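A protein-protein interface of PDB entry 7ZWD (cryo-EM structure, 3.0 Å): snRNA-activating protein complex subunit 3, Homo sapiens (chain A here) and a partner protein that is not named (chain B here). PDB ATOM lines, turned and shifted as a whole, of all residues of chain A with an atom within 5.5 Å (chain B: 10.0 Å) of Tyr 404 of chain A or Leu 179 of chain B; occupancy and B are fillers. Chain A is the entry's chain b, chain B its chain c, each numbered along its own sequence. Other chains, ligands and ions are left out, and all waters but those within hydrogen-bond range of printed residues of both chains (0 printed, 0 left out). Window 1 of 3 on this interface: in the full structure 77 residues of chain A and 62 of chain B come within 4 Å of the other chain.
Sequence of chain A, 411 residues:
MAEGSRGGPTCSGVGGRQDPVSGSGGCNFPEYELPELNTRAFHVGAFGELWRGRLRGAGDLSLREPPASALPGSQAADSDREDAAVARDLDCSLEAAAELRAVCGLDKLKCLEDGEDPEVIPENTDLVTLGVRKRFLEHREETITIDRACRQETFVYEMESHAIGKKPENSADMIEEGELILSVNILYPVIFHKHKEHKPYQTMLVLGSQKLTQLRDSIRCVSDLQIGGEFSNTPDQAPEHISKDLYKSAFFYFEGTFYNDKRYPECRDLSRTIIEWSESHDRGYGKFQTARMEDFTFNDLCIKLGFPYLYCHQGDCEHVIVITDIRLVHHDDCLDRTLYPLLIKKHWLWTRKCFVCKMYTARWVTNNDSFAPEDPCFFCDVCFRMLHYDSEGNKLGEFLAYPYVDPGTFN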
ATOM      1  N   GLN A 226      -4.640  18.358   4.922  1.00  0.00           N
ATOM      2  CA  GLN A 226      -3.669  17.310   5.178  1.00  0.00           C
ATOM      3  C   GLN A 226      -3.195  16.706   3.868  1.00  0.00           C
ATOM      4  O   GLN A 226      -3.988  16.489   2.950  1.00  0.00           O
ATOM      5  CB  GLN A 226      -4.275  16.238   6.071  1.00  0.00           C
ATOM      6  CG  GLN A 226      -4.410  16.668   7.504  1.00  0.00           C
ATOM      7  CD  GLN A 226      -5.184  15.676   8.324  1.00  0.00           C
ATOM      8  OE1 GLN A 226      -6.137  15.071   7.840  1.00  0.00           O
ATOM      9  NE2 GLN A 226      -4.785  15.500   9.576  1.00  0.00           N
ATOM     10  N   ARG A 352       2.063  22.947  17.717  1.00  0.00           N
ATOM     11  CA  ARG A 352       3.162  22.028  17.972  1.00  0.00           C
ATOM     12  C   ARG A 352       4.454  22.643  17.472  1.00  0.00           C
ATOM     13  O   ARG A 352       4.450  23.422  16.520  1.00  0.00           O
ATOM     14  CB  ARG A 352       2.919  20.694  17.276  1.00  0.00           C
ATOM     15  CG  ARG A 352       2.301  19.608  18.133  1.00  0.00           C
ATOM     16  CD  ARG A 352       0.830  19.847  18.346  1.00  0.00           C
ATOM     17  NE  ARG A 352       0.148  18.691  18.918  1.00  0.00           N
ATOM     18  CZ  ARG A 352      -0.581  17.830  18.220  1.00  0.00           C
ATOM     19  NH1 ARG A 352      -0.742  17.994  16.918  1.00  0.00           N
ATOM     20  NH2 ARG A 352      -1.169  16.814  18.827  1.00  0.00           N
ATOM     21  N   ALA A 362       6.234  22.433  13.758  1.00  0.00           N
ATOM     22  CA  ALA A 362       6.417  21.112  13.187  1.00  0.00           C
ATOM     23  C   ALA A 362       5.902  21.052  11.766  1.00  0.00           C
ATOM     24  O   ALA A 362       4.716  21.271  11.516  1.00  0.00           O
ATOM     25  CB  ALA A 362       5.687  20.091  14.046  1.00  0.00           C
ATOM     26  N   ARG A 363       6.789  20.735  10.834  1.00  0.00           N
ATOM     27  CA  ARG A 363       6.377  20.447   9.476  1.00  0.00           C
ATOM     28  C   ARG A 363       6.212  18.960   9.233  1.00  0.00           C
ATOM     29  O   ARG A 363       5.427  18.574   8.362  1.00  0.00           O
ATOM     30  CB  ARG A 363       7.385  21.006   8.468  1.00  0.00           C
ATOM     31  CG  ARG A 363       7.752  22.446   8.677  1.00  0.00           C
ATOM     32  CD  ARG A 363       6.603  23.354   8.354  1.00  0.00           C
ATOM     33  NE  ARG A 363       6.980  24.754   8.473  1.00  0.00           N
ATOM     34  CZ  ARG A 363       7.288  25.523   7.441  1.00  0.00           C
ATOM     35  NH1 ARG A 363       7.243  25.024   6.217  1.00  0.00           N
ATOM     36  NH2 ARG A 363       7.626  26.789   7.625  1.00  0.00           N
ATOM     37  N   TRP A 364       6.905  18.115   9.989  1.00  0.00           N
ATOM     38  CA  TRP A 364       6.934  16.685   9.732  1.00  0.00           C
ATOM     39  C   TRP A 364       6.586  15.935  10.998  1.00  0.00           C
ATOM     40  O   TRP A 364       6.891  16.402  12.093  1.00  0.00           O
ATOM     41  CB  TRP A 364       8.307  16.252   9.252  1.00  0.00           C
ATOM     42  CG  TRP A 364       8.678  16.860   7.978  1.00  0.00           C
ATOM     43  CD1 TRP A 364       9.384  17.999   7.798  1.00  0.00           C
ATOM     44  CD2 TRP A 364       8.370  16.365   6.681  1.00  0.00           C
ATOM     45  NE1 TRP A 364       9.536  18.253   6.465  1.00  0.00           N
ATOM     46  CE2 TRP A 364       8.919  17.258   5.756  1.00  0.00           C
ATOM     47  CE3 TRP A 364       7.684  15.248   6.213  1.00  0.00           C
ATOM     48  CZ2 TRP A 364       8.804  17.072   4.394  1.00  0.00           C
ATOM     49  CZ3 TRP A 364       7.570  15.068   4.867  1.00  0.00           C
ATOM     50  CH2 TRP A 364       8.127  15.971   3.970  1.00  0.00           C
ATOM     51  N   VAL A 365       5.964  14.775  10.848  1.00  0.00           N
ATOM     52  CA  VAL A 365       5.752  13.842  11.944  1.00  0.00           C
ATOM     53  C   VAL A 365       6.297  12.490  11.522  1.00  0.00           C
ATOM     54  O   VAL A 365       5.950  11.982  10.454  1.00  0.00           O
ATOM     55  CB  VAL A 365       4.269  13.756  12.341  1.00  0.00           C
ATOM     56  CG1 VAL A 365       3.414  13.445  11.153  1.00  0.00           C
ATOM     57  CG2 VAL A 365       4.082  12.683  13.371  1.00  0.00           C
ATOM     58  N   PRO A 376       5.569   9.297  17.877  1.00  0.00           N
ATOM     59  CA  PRO A 376       5.266  10.337  16.895  1.00  0.00           C
ATOM     60  C   PRO A 376       6.092  11.559  17.213  1.00  0.00           C
ATOM     61  O   PRO A 376       5.772  12.291  18.148  1.00  0.00           O
ATOM     62  CB  PRO A 376       3.769  10.584  17.090  1.00  0.00           C
ATOM     63  CG  PRO A 376       3.533  10.282  18.503  1.00  0.00           C
ATOM     64  CD  PRO A 376       4.581   9.308  18.971  1.00  0.00           C
ATOM     65  N   PHE A 378       7.641  15.200  16.137  1.00  0.00           N
ATOM     66  CA  PHE A 378       7.392  16.300  15.225  1.00  0.00           C
ATOM     67  C   PHE A 378       8.664  17.100  15.026  1.00  0.00           C
ATOM     68  O   PHE A 378       9.373  17.400  15.986  1.00  0.00           O
ATOM     69  CB  PHE A 378       6.295  17.204  15.766  1.00  0.00           C
ATOM     70  CG  PHE A 378       5.041  16.487  16.109  1.00  0.00           C
ATOM     71  CD1 PHE A 378       4.056  16.312  15.177  1.00  0.00           C
ATOM     72  CD2 PHE A 378       4.842  15.999  17.367  1.00  0.00           C
ATOM     73  CE1 PHE A 378       2.908  15.657  15.493  1.00  0.00           C
ATOM     74  CE2 PHE A 378       3.692  15.342  17.684  1.00  0.00           C
ATOM     75  CZ  PHE A 378       2.726  15.171  16.744  1.00  0.00           C
ATOM     76  N   TYR A 402       5.747  11.689   7.599  1.00  0.00           N
ATOM     77  CA  TYR A 402       4.590  12.265   6.958  1.00  0.00           C
ATOM     78  C   TYR A 402       4.638  13.776   7.097  1.00  0.00           C
ATOM     79  O   TYR A 402       5.186  14.294   8.072  1.00  0.00           O
ATOM     80  CB  TYR A 402       3.293  11.743   7.578  1.00  0.00           C
ATOM     81  CG  TYR A 402       3.246  10.253   7.717  1.00  0.00           C
ATOM     82  CD1 TYR A 402       2.550   9.480   6.815  1.00  0.00           C
ATOM     83  CD2 TYR A 402       3.892   9.617   8.756  1.00  0.00           C
ATOM     84  CE1 TYR A 402       2.503   8.118   6.939  1.00  0.00           C
ATOM     85  CE2 TYR A 402       3.855   8.261   8.887  1.00  0.00           C
ATOM     86  CZ  TYR A 402       3.157   7.513   7.979  1.00  0.00           C
ATOM     87  OH  TYR A 402       3.112   6.148   8.107  1.00  0.00           O
ATOM     88  N   PRO A 403       4.096  14.511   6.137  1.00  0.00           N
ATOM     89  CA  PRO A 403       4.007  15.958   6.299  1.00  0.00           C
ATOM     90  C   PRO A 403       2.925  16.292   7.305  1.00  0.00           C
ATOM     91  O   PRO A 403       1.854  15.682   7.322  1.00  0.00           O
ATOM     92  CB  PRO A 403       3.645  16.442   4.897  1.00  0.00           C
ATOM     93  CG  PRO A 403       2.887  15.323   4.329  1.00  0.00           C
ATOM     94  CD  PRO A 403       3.482  14.065   4.878  1.00  0.00           C
ATOM     95  N   TYR A 404       3.215  17.269   8.152  1.00  0.00           N
ATOM     96  CA  TYR A 404       2.347  17.605   9.266  1.00  0.00           C
ATOM     97  C   TYR A 404       1.846  19.028   9.112  1.00  0.00           C
ATOM     98  O   TYR A 404       2.637  19.972   9.151  1.00  0.00           O
ATOM     99  CB  TYR A 404       3.094  17.449  10.582  1.00  0.00           C
ATOM    100  CG  TYR A 404       2.315  17.861  11.791  1.00  0.00           C
ATOM    101  CD1 TYR A 404       1.128  17.246  12.113  1.00  0.00           C
ATOM    102  CD2 TYR A 404       2.775  18.863  12.617  1.00  0.00           C
ATOM    103  CE1 TYR A 404       0.423  17.619  13.217  1.00  0.00           C
ATOM    104  CE2 TYR A 404       2.079  19.241  13.717  1.00  0.00           C
ATOM    105  CZ  TYR A 404       0.903  18.617  14.012  1.00  0.00           C
ATOM    106  OH  TYR A 404       0.199  18.992  15.124  1.00  0.00           O
ATOM    107  N   VAL A 405       0.539  19.179   8.934  1.00  0.00           N
ATOM    108  CA  VAL A 405      -0.106  20.483   8.907  1.00  0.00           C
ATOM    109  C   VAL A 405      -0.472  20.837  10.336  1.00  0.00           C
ATOM    110  O   VAL A 405      -1.261  20.135  10.977  1.00  0.00           O
ATOM    111  CB  VAL A 405      -1.340  20.491   7.999  1.00  0.00           C
ATOM    112  CG1 VAL A 405      -0.908  20.512   6.566  1.00  0.00           C
ATOM    113  CG2 VAL A 405      -2.175  19.275   8.259  1.00  0.00           C
ATOM    114  N   ASP A 406       0.104  21.901  10.836  1.00  0.00           N
ATOM    115  CA  ASP A 406      -0.101  22.272  12.224  1.00  0.00           C
ATOM    116  C   ASP A 406      -1.532  22.747  12.428  1.00  0.00           C
ATOM    117  O   ASP A 406      -1.930  23.750  11.839  1.00  0.00           O
ATOM    118  CB  ASP A 406       0.867  23.364  12.612  1.00  0.00           C
ATOM    119  CG  ASP A 406       1.024  23.490  14.084  1.00  0.00           C
ATOM    120  OD1 ASP A 406       0.430  22.681  14.816  1.00  0.00           O
ATOM    121  OD2 ASP A 406       1.747  24.401  14.514  1.00  0.00           O
ATOM    122  N   PRO A 407      -2.331  22.059  13.240  1.00  0.00           N
ATOM    123  CA  PRO A 407      -3.715  22.496  13.435  1.00  0.00           C
ATOM    124  C   PRO A 407      -3.829  23.852  14.083  1.00  0.00           C
ATOM    125  O   PRO A 407      -4.785  24.574  13.796  1.00  0.00           O
ATOM    126  CB  PRO A 407      -4.306  21.407  14.333  1.00  0.00           C
ATOM    127  CG  PRO A 407      -3.398  20.260  14.196  1.00  0.00           C
ATOM    128  CD  PRO A 407      -2.047  20.827  13.981  1.00  0.00           C
ATOM    129  N   LYS B 168      -8.761   7.406   2.898  1.00  0.00           N
ATOM    130  CA  LYS B 168      -7.903   8.357   3.588  1.00  0.00           C
ATOM    131  C   LYS B 168      -6.889   7.641   4.462  1.00  0.00           C
ATOM    132  O   LYS B 168      -5.711   8.010   4.490  1.00  0.00           O
ATOM    133  CB  LYS B 168      -8.764   9.294   4.429  1.00  0.00           C
ATOM    134  CG  LYS B 168      -8.178  10.652   4.686  1.00  0.00           C
ATOM    135  CD  LYS B 168      -9.099  11.443   5.588  1.00  0.00           C
ATOM    136  CE  LYS B 168      -8.534  12.808   5.884  1.00  0.00           C
ATOM    137  NZ  LYS B 168      -8.599  13.676   4.687  1.00  0.00           N
ATOM    138  N   GLY B 172      -2.297   6.950   4.506  1.00  0.00           N
ATOM    139  CA  GLY B 172      -1.462   7.280   5.643  1.00  0.00           C
ATOM    140  C   GLY B 172      -1.683   8.676   6.177  1.00  0.00           C
ATOM    141  O   GLY B 172      -0.732   9.313   6.646  1.00  0.00           O
ATOM    142  N   ILE B 173      -2.913   9.173   6.115  1.00  0.00           N
ATOM    143  CA  ILE B 173      -3.255  10.475   6.668  1.00  0.00           C
ATOM    144  C   ILE B 173      -3.583  10.254   8.138  1.00  0.00           C
ATOM    145  O   ILE B 173      -4.618   9.681   8.478  1.00  0.00           O
ATOM    146  CB  ILE B 173      -4.409  11.129   5.912  1.00  0.00           C
ATOM    147  CG1 ILE B 173      -3.916  11.659   4.573  1.00  0.00           C
ATOM    148  CG2 ILE B 173      -4.982  12.260   6.712  1.00  0.00           C
ATOM    149  CD1 ILE B 173      -4.986  12.289   3.748  1.00  0.00           C
ATOM    150  N   LYS B 174      -2.683  10.698   9.010  1.00  0.00           N
ATOM    151  CA  LYS B 174      -2.839  10.483  10.438  1.00  0.00           C
ATOM    152  C   LYS B 174      -4.095  11.166  10.951  1.00  0.00           C
ATOM    153  O   LYS B 174      -4.300  12.362  10.741  1.00  0.00           O
ATOM    154  CB  LYS B 174      -1.624  11.019  11.188  1.00  0.00           C
ATOM    155  CG  LYS B 174      -0.324  10.342  10.842  1.00  0.00           C
ATOM    156  CD  LYS B 174      -0.377   8.878  11.188  1.00  0.00           C
ATOM    157  CE  LYS B 174       0.781   8.128  10.573  1.00  0.00           C
ATOM    158  NZ  LYS B 174       0.570   6.657  10.643  1.00  0.00           N
ATOM    159  N   ALA B 175      -4.942  10.400  11.627  1.00  0.00           N
ATOM    160  CA  ALA B 175      -6.072  11.001  12.305  1.00  0.00           C
ATOM    161  C   ALA B 175      -5.581  11.860  13.462  1.00  0.00           C
ATOM    162  O   ALA B 175      -4.408  11.833  13.835  1.00  0.00           O
ATOM    163  CB  ALA B 175      -7.032   9.930  12.812  1.00  0.00           C
ATOM    164  N   PHE B 176      -6.496  12.640  14.032  1.00  0.00           N
ATOM    165  CA  PHE B 176      -6.109  13.547  15.105  1.00  0.00           C
ATOM    166  C   PHE B 176      -5.597  12.783  16.312  1.00  0.00           C
ATOM    167  O   PHE B 176      -4.626  13.200  16.951  1.00  0.00           O
ATOM    168  CB  PHE B 176      -7.286  14.430  15.494  1.00  0.00           C
ATOM    169  CG  PHE B 176      -7.566  15.516  14.516  1.00  0.00           C
ATOM    170  CD1 PHE B 176      -6.560  16.354  14.095  1.00  0.00           C
ATOM    171  CD2 PHE B 176      -8.834  15.703  14.022  1.00  0.00           C
ATOM    172  CE1 PHE B 176      -6.814  17.349  13.198  1.00  0.00           C
ATOM    173  CE2 PHE B 176      -9.087  16.700  13.127  1.00  0.00           C
ATOM    174  CZ  PHE B 176      -8.079  17.523  12.716  1.00  0.00           C
ATOM    175  N   GLU B 177      -6.229  11.658  16.637  1.00  0.00           N
ATOM    176  CA  GLU B 177      -5.826  10.902  17.812  1.00  0.00           C
ATOM    177  C   GLU B 177      -4.540  10.122  17.589  1.00  0.00           C
ATOM    178  O   GLU B 177      -4.011   9.546  18.541  1.00  0.00           O
ATOM    179  CB  GLU B 177      -6.943   9.956  18.238  1.00  0.00           C
ATOM    180  CG  GLU B 177      -7.228   8.859  17.250  1.00  0.00           C
ATOM    181  CD  GLU B 177      -8.352   9.214  16.307  1.00  0.00           C
ATOM    182  OE1 GLU B 177      -8.998  10.260  16.519  1.00  0.00           O
ATOM    183  OE2 GLU B 177      -8.589   8.446  15.354  1.00  0.00           O
ATOM    184  N   GLU B 178      -4.023  10.086  16.364  1.00  0.00           N
ATOM    185  CA  GLU B 178      -2.734   9.451  16.141  1.00  0.00           C
ATOM    186  C   GLU B 178      -1.586  10.433  16.301  1.00  0.00           C
ATOM    187  O   GLU B 178      -0.506  10.047  16.757  1.00  0.00           O
ATOM    188  CB  GLU B 178      -2.684   8.812  14.755  1.00  0.00           C
ATOM    189  CG  GLU B 178      -3.830   7.867  14.466  1.00  0.00           C
ATOM    190  CD  GLU B 178      -3.829   7.369  13.032  1.00  0.00           C
ATOM    191  OE1 GLU B 178      -4.821   7.613  12.316  1.00  0.00           O
ATOM    192  OE2 GLU B 178      -2.838   6.733  12.620  1.00  0.00           O
ATOM    193  N   LEU B 179      -1.791  11.693  15.930  1.00  0.00           N
ATOM    194  CA  LEU B 179      -0.804  12.739  16.141  1.00  0.00           C
ATOM    195  C   LEU B 179      -0.849  13.288  17.550  1.00  0.00           C
ATOM    196  O   LEU B 179      -0.231  14.321  17.825  1.00  0.00           O
ATOM    197  CB  LEU B 179      -1.017  13.876  15.149  1.00  0.00           C
ATOM    198  CG  LEU B 179      -0.954  13.502  13.681  1.00  0.00           C
ATOM    199  CD1 LEU B 179      -1.632  14.564  12.857  1.00  0.00           C
ATOM    200  CD2 LEU B 179       0.476  13.338  13.254  1.00  0.00           C
ATOM    201  N   LEU B 180      -1.570  12.630  18.441  1.00  0.00           N
ATOM    202  CA  LEU B 180      -1.825  13.173  19.762  1.00  0.00           C
ATOM    203  C   LEU B 180      -0.697  12.767  20.695  1.00  0.00           C
ATOM    204  O   LEU B 180      -0.517  11.583  20.988  1.00  0.00           O
ATOM    205  CB  LEU B 180      -3.172  12.669  20.260  1.00  0.00           C
ATOM    206  CG  LEU B 180      -3.855  13.380  21.408  1.00  0.00           C
ATOM    207  CD1 LEU B 180      -5.342  13.248  21.203  1.00  0.00           C
ATOM    208  CD2 LEU B 180      -3.451  12.757  22.714  1.00  0.00           C
ATOM    209  N   VAL B 181       0.064  13.752  21.157  1.00  0.00           N
ATOM    210  CA  VAL B 181       1.276  13.523  21.929  1.00  0.00           C
ATOM    211  C   VAL B 181       1.016  13.908  23.376  1.00  0.00           C
ATOM    212  O   VAL B 181       0.307  14.880  23.652  1.00  0.00           O
ATOM    213  CB  VAL B 181       2.466  14.318  21.355  1.00  0.00           C
ATOM    214  CG1 VAL B 181       2.131  15.790  21.287  1.00  0.00           C
ATOM    215  CG2 VAL B 181       3.710  14.097  22.185  1.00  0.00           C
ATOM    216  N   THR B 182       1.573  13.129  24.298  1.00  0.00           N
ATOM    217  CA  THR B 182       1.494  13.413  25.722  1.00  0.00           C
ATOM    218  C   THR B 182       2.857  13.195  26.356  1.00  0.00           C
ATOM    219  O   THR B 182       3.585  12.277  25.972  1.00  0.00           O
ATOM    220  CB  THR B 182       0.435  12.547  26.401  1.00  0.00           C
ATOM    221  OG1 THR B 182       0.459  12.777  27.813  1.00  0.00           O
ATOM    222  CG2 THR B 182       0.662  11.089  26.107  1.00  0.00           C
ATOM    223  N   GLU B 279       5.038   3.304  21.134  1.00  0.00           N
ATOM    224  CA  GLU B 279       5.386   4.459  21.947  1.00  0.00           C
ATOM    225  C   GLU B 279       6.339   4.065  23.064  1.00  0.00           C
ATOM    226  O   GLU B 279       7.411   4.661  23.221  1.00  0.00           O
ATOM    227  CB  GLU B 279       4.117   5.082  22.512  1.00  0.00           C
ATOM    228  CG  GLU B 279       4.339   6.310  23.343  1.00  0.00           C
ATOM    229  CD  GLU B 279       3.144   7.228  23.310  1.00  0.00           C
ATOM    230  OE1 GLU B 279       3.316   8.445  23.527  1.00  0.00           O
ATOM    231  OE2 GLU B 279       2.028   6.730  23.055  1.00  0.00           O
ATOM    232  N   ARG B 373       2.802  33.787  15.979  1.00  0.00           N
ATOM    233  CA  ARG B 373       3.148  32.379  15.881  1.00  0.00           C
ATOM    234  C   ARG B 373       2.551  31.754  14.629  1.00  0.00           C
ATOM    235  O   ARG B 373       3.076  30.770  14.105  1.00  0.00           O
ATOM    236  CB  ARG B 373       2.691  31.647  17.130  1.00  0.00           C
ATOM    237  CG  ARG B 373       3.602  31.897  18.295  1.00  0.00           C
ATOM    238  CD  ARG B 373       4.953  31.311  18.031  1.00  0.00           C
ATOM    239  NE  ARG B 373       4.860  29.874  17.855  1.00  0.00           N
ATOM    240  CZ  ARG B 373       5.842  29.118  17.391  1.00  0.00           C
ATOM    241  NH1 ARG B 373       6.992  29.665  17.037  1.00  0.00           N
ATOM    242  NH2 ARG B 373       5.657  27.817  17.266  1.00  0.00           N
ATOM    243  N   TYR B 377       5.333  30.844  10.586  1.00  0.00           N
ATOM    244  CA  TYR B 377       5.454  29.616   9.821  1.00  0.00           C
ATOM    245  C   TYR B 377       5.447  29.865   8.329  1.00  0.00           C
ATOM    246  O   TYR B 377       5.412  28.903   7.557  1.00  0.00           O
ATOM    247  CB  TYR B 377       4.350  28.640  10.220  1.00  0.00           C
ATOM    248  CG  TYR B 377       4.240  28.437  11.726  1.00  0.00           C
ATOM    249  CD1 TYR B 377       5.277  28.798  12.591  1.00  0.00           C
ATOM    250  CD2 TYR B 377       3.107  27.877  12.288  1.00  0.00           C
ATOM    251  CE1 TYR B 377       5.170  28.619  13.966  1.00  0.00           C
ATOM    252  CE2 TYR B 377       2.998  27.696  13.654  1.00  0.00           C
ATOM    253  CZ  TYR B 377       4.024  28.063  14.487  1.00  0.00           C
ATOM    254  OH  TYR B 377       3.891  27.864  15.839  1.00  0.00           O
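The backbone carbonyl oxygen (O) of Tyr 377 of chain B is in hydrogen-bond range of the guanidinium group (NH2) of Arg 363 of chain A (3.1 Å).
The side-chain amide nitrogen (NE2) of Gln 226 of chain A lies within hydrogen-bond range of the backbone carbonyl oxygen (O) of Lys 174 of chain B (3.4 Å).
The guanidinium group (NH2) of Arg 352 of chain A is in hydrogen-bond range of the backbone carbonyl oxygen (O) of Leu 179 of chain B (2.8 Å).
The backbone carbonyl oxygen (O) of Arg 363 of chain A lies within hydrogen-bond range of the backbone NH (N) of Tyr 404 of chain A (2.6 Å).
The backbone carbonyl oxygen of Arg 352 of chain A sits at hydrogen-bond distance from the backbone NH of Ala 362 of chain A (3.4 Å).
The backbone NH of Arg 352 of chain A lies within hydrogen-bond range of the side-chain carboxylate of Asp 406 of chain A (3.3 Å).
NZ of Lys 174 of chain B lies within salt-bridge range of OE2 of Glu 178 of chain B.
N of Tyr 402 of chain A is in hydrogen-bond range of O of Val 365 of chain A, at 2.9 Å.
The backbone carbonyl oxygen of Lys 168 of chain B sits at hydrogen-bond distance from the backbone NH of Ile 173 of chain B (3.4 Å).
OE1 of Gln 226 of chain A touches CE of Lys 168 of chain B, at 3.8 Å.
OE1 of Gln 226 of chain A touches CG2 of Ile 173 of chain B, at 3.2 Å.
CA of Leu 180 of chain B touches NH2 of Arg 352 of chain A, at 3.8 Å.
CG1 of Val 365 of chain A touches CD2 of Leu 179 of chain B (3.6 Å).
O of Leu 179 of chain B touches CZ of Phe 378 of chain A (3.3 Å).
CG1 of Val 181 of chain B touches CE2 of Phe 378 of chain A, at 3.95 Å.
Tyr 402 of chain A touches Gly 172 of chain B (CD1 to O, 3.3 Å).
Lys 174 of chain B touches Tyr 402 of chain A (CE to CE2, 3.5 Å).
CE1 of Tyr 404 of chain A touches CD1 of Leu 179 of chain B, 3.7 Å away.
Tyr 377 of chain B touches Asp 406 of chain A.
No residue of chain B comes within 4 Å of Ala 362 of chain A.
No residue of chain B comes within 4 Å of Pro 403 of chain A.
Of chain B, only Leu 179 (3.7 Å) comes within 4 Å of Tyr 404 of chain A.
No residue of chain B comes within 4 Å of Val 405 of chain A.
Of the printed residues of chain A, Lys 168 of chain B touches Gln 226 (3.8 Å).
Of chain A, only Arg 352 (2.8 Å), Val 365 (3.6 Å), Phe 378 (3.3 Å) and Tyr 404 (3.7 Å) come within 4 Å of Leu 179 of chain B.
Printed residues of chain A within 4 Å of Val 181 of chain B: Phe 378 (3.95 Å).
The nearest residue of chain B that does not touch Tyr 404 of chain A is Lys 174 of chain B (6.9 Å).
Hydrophobic or aromatic side chains of chain B within 4 Å of the printed part of chain A: Ile 173, Leu 179, Val 181 and Tyr 377.
Among the printed residues, 13 pairs touch across the chains.
Among the printed residues, no Asp or Glu carboxylate lies within 4 Å of a Lys or Arg side-chain nitrogen of the other chain.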
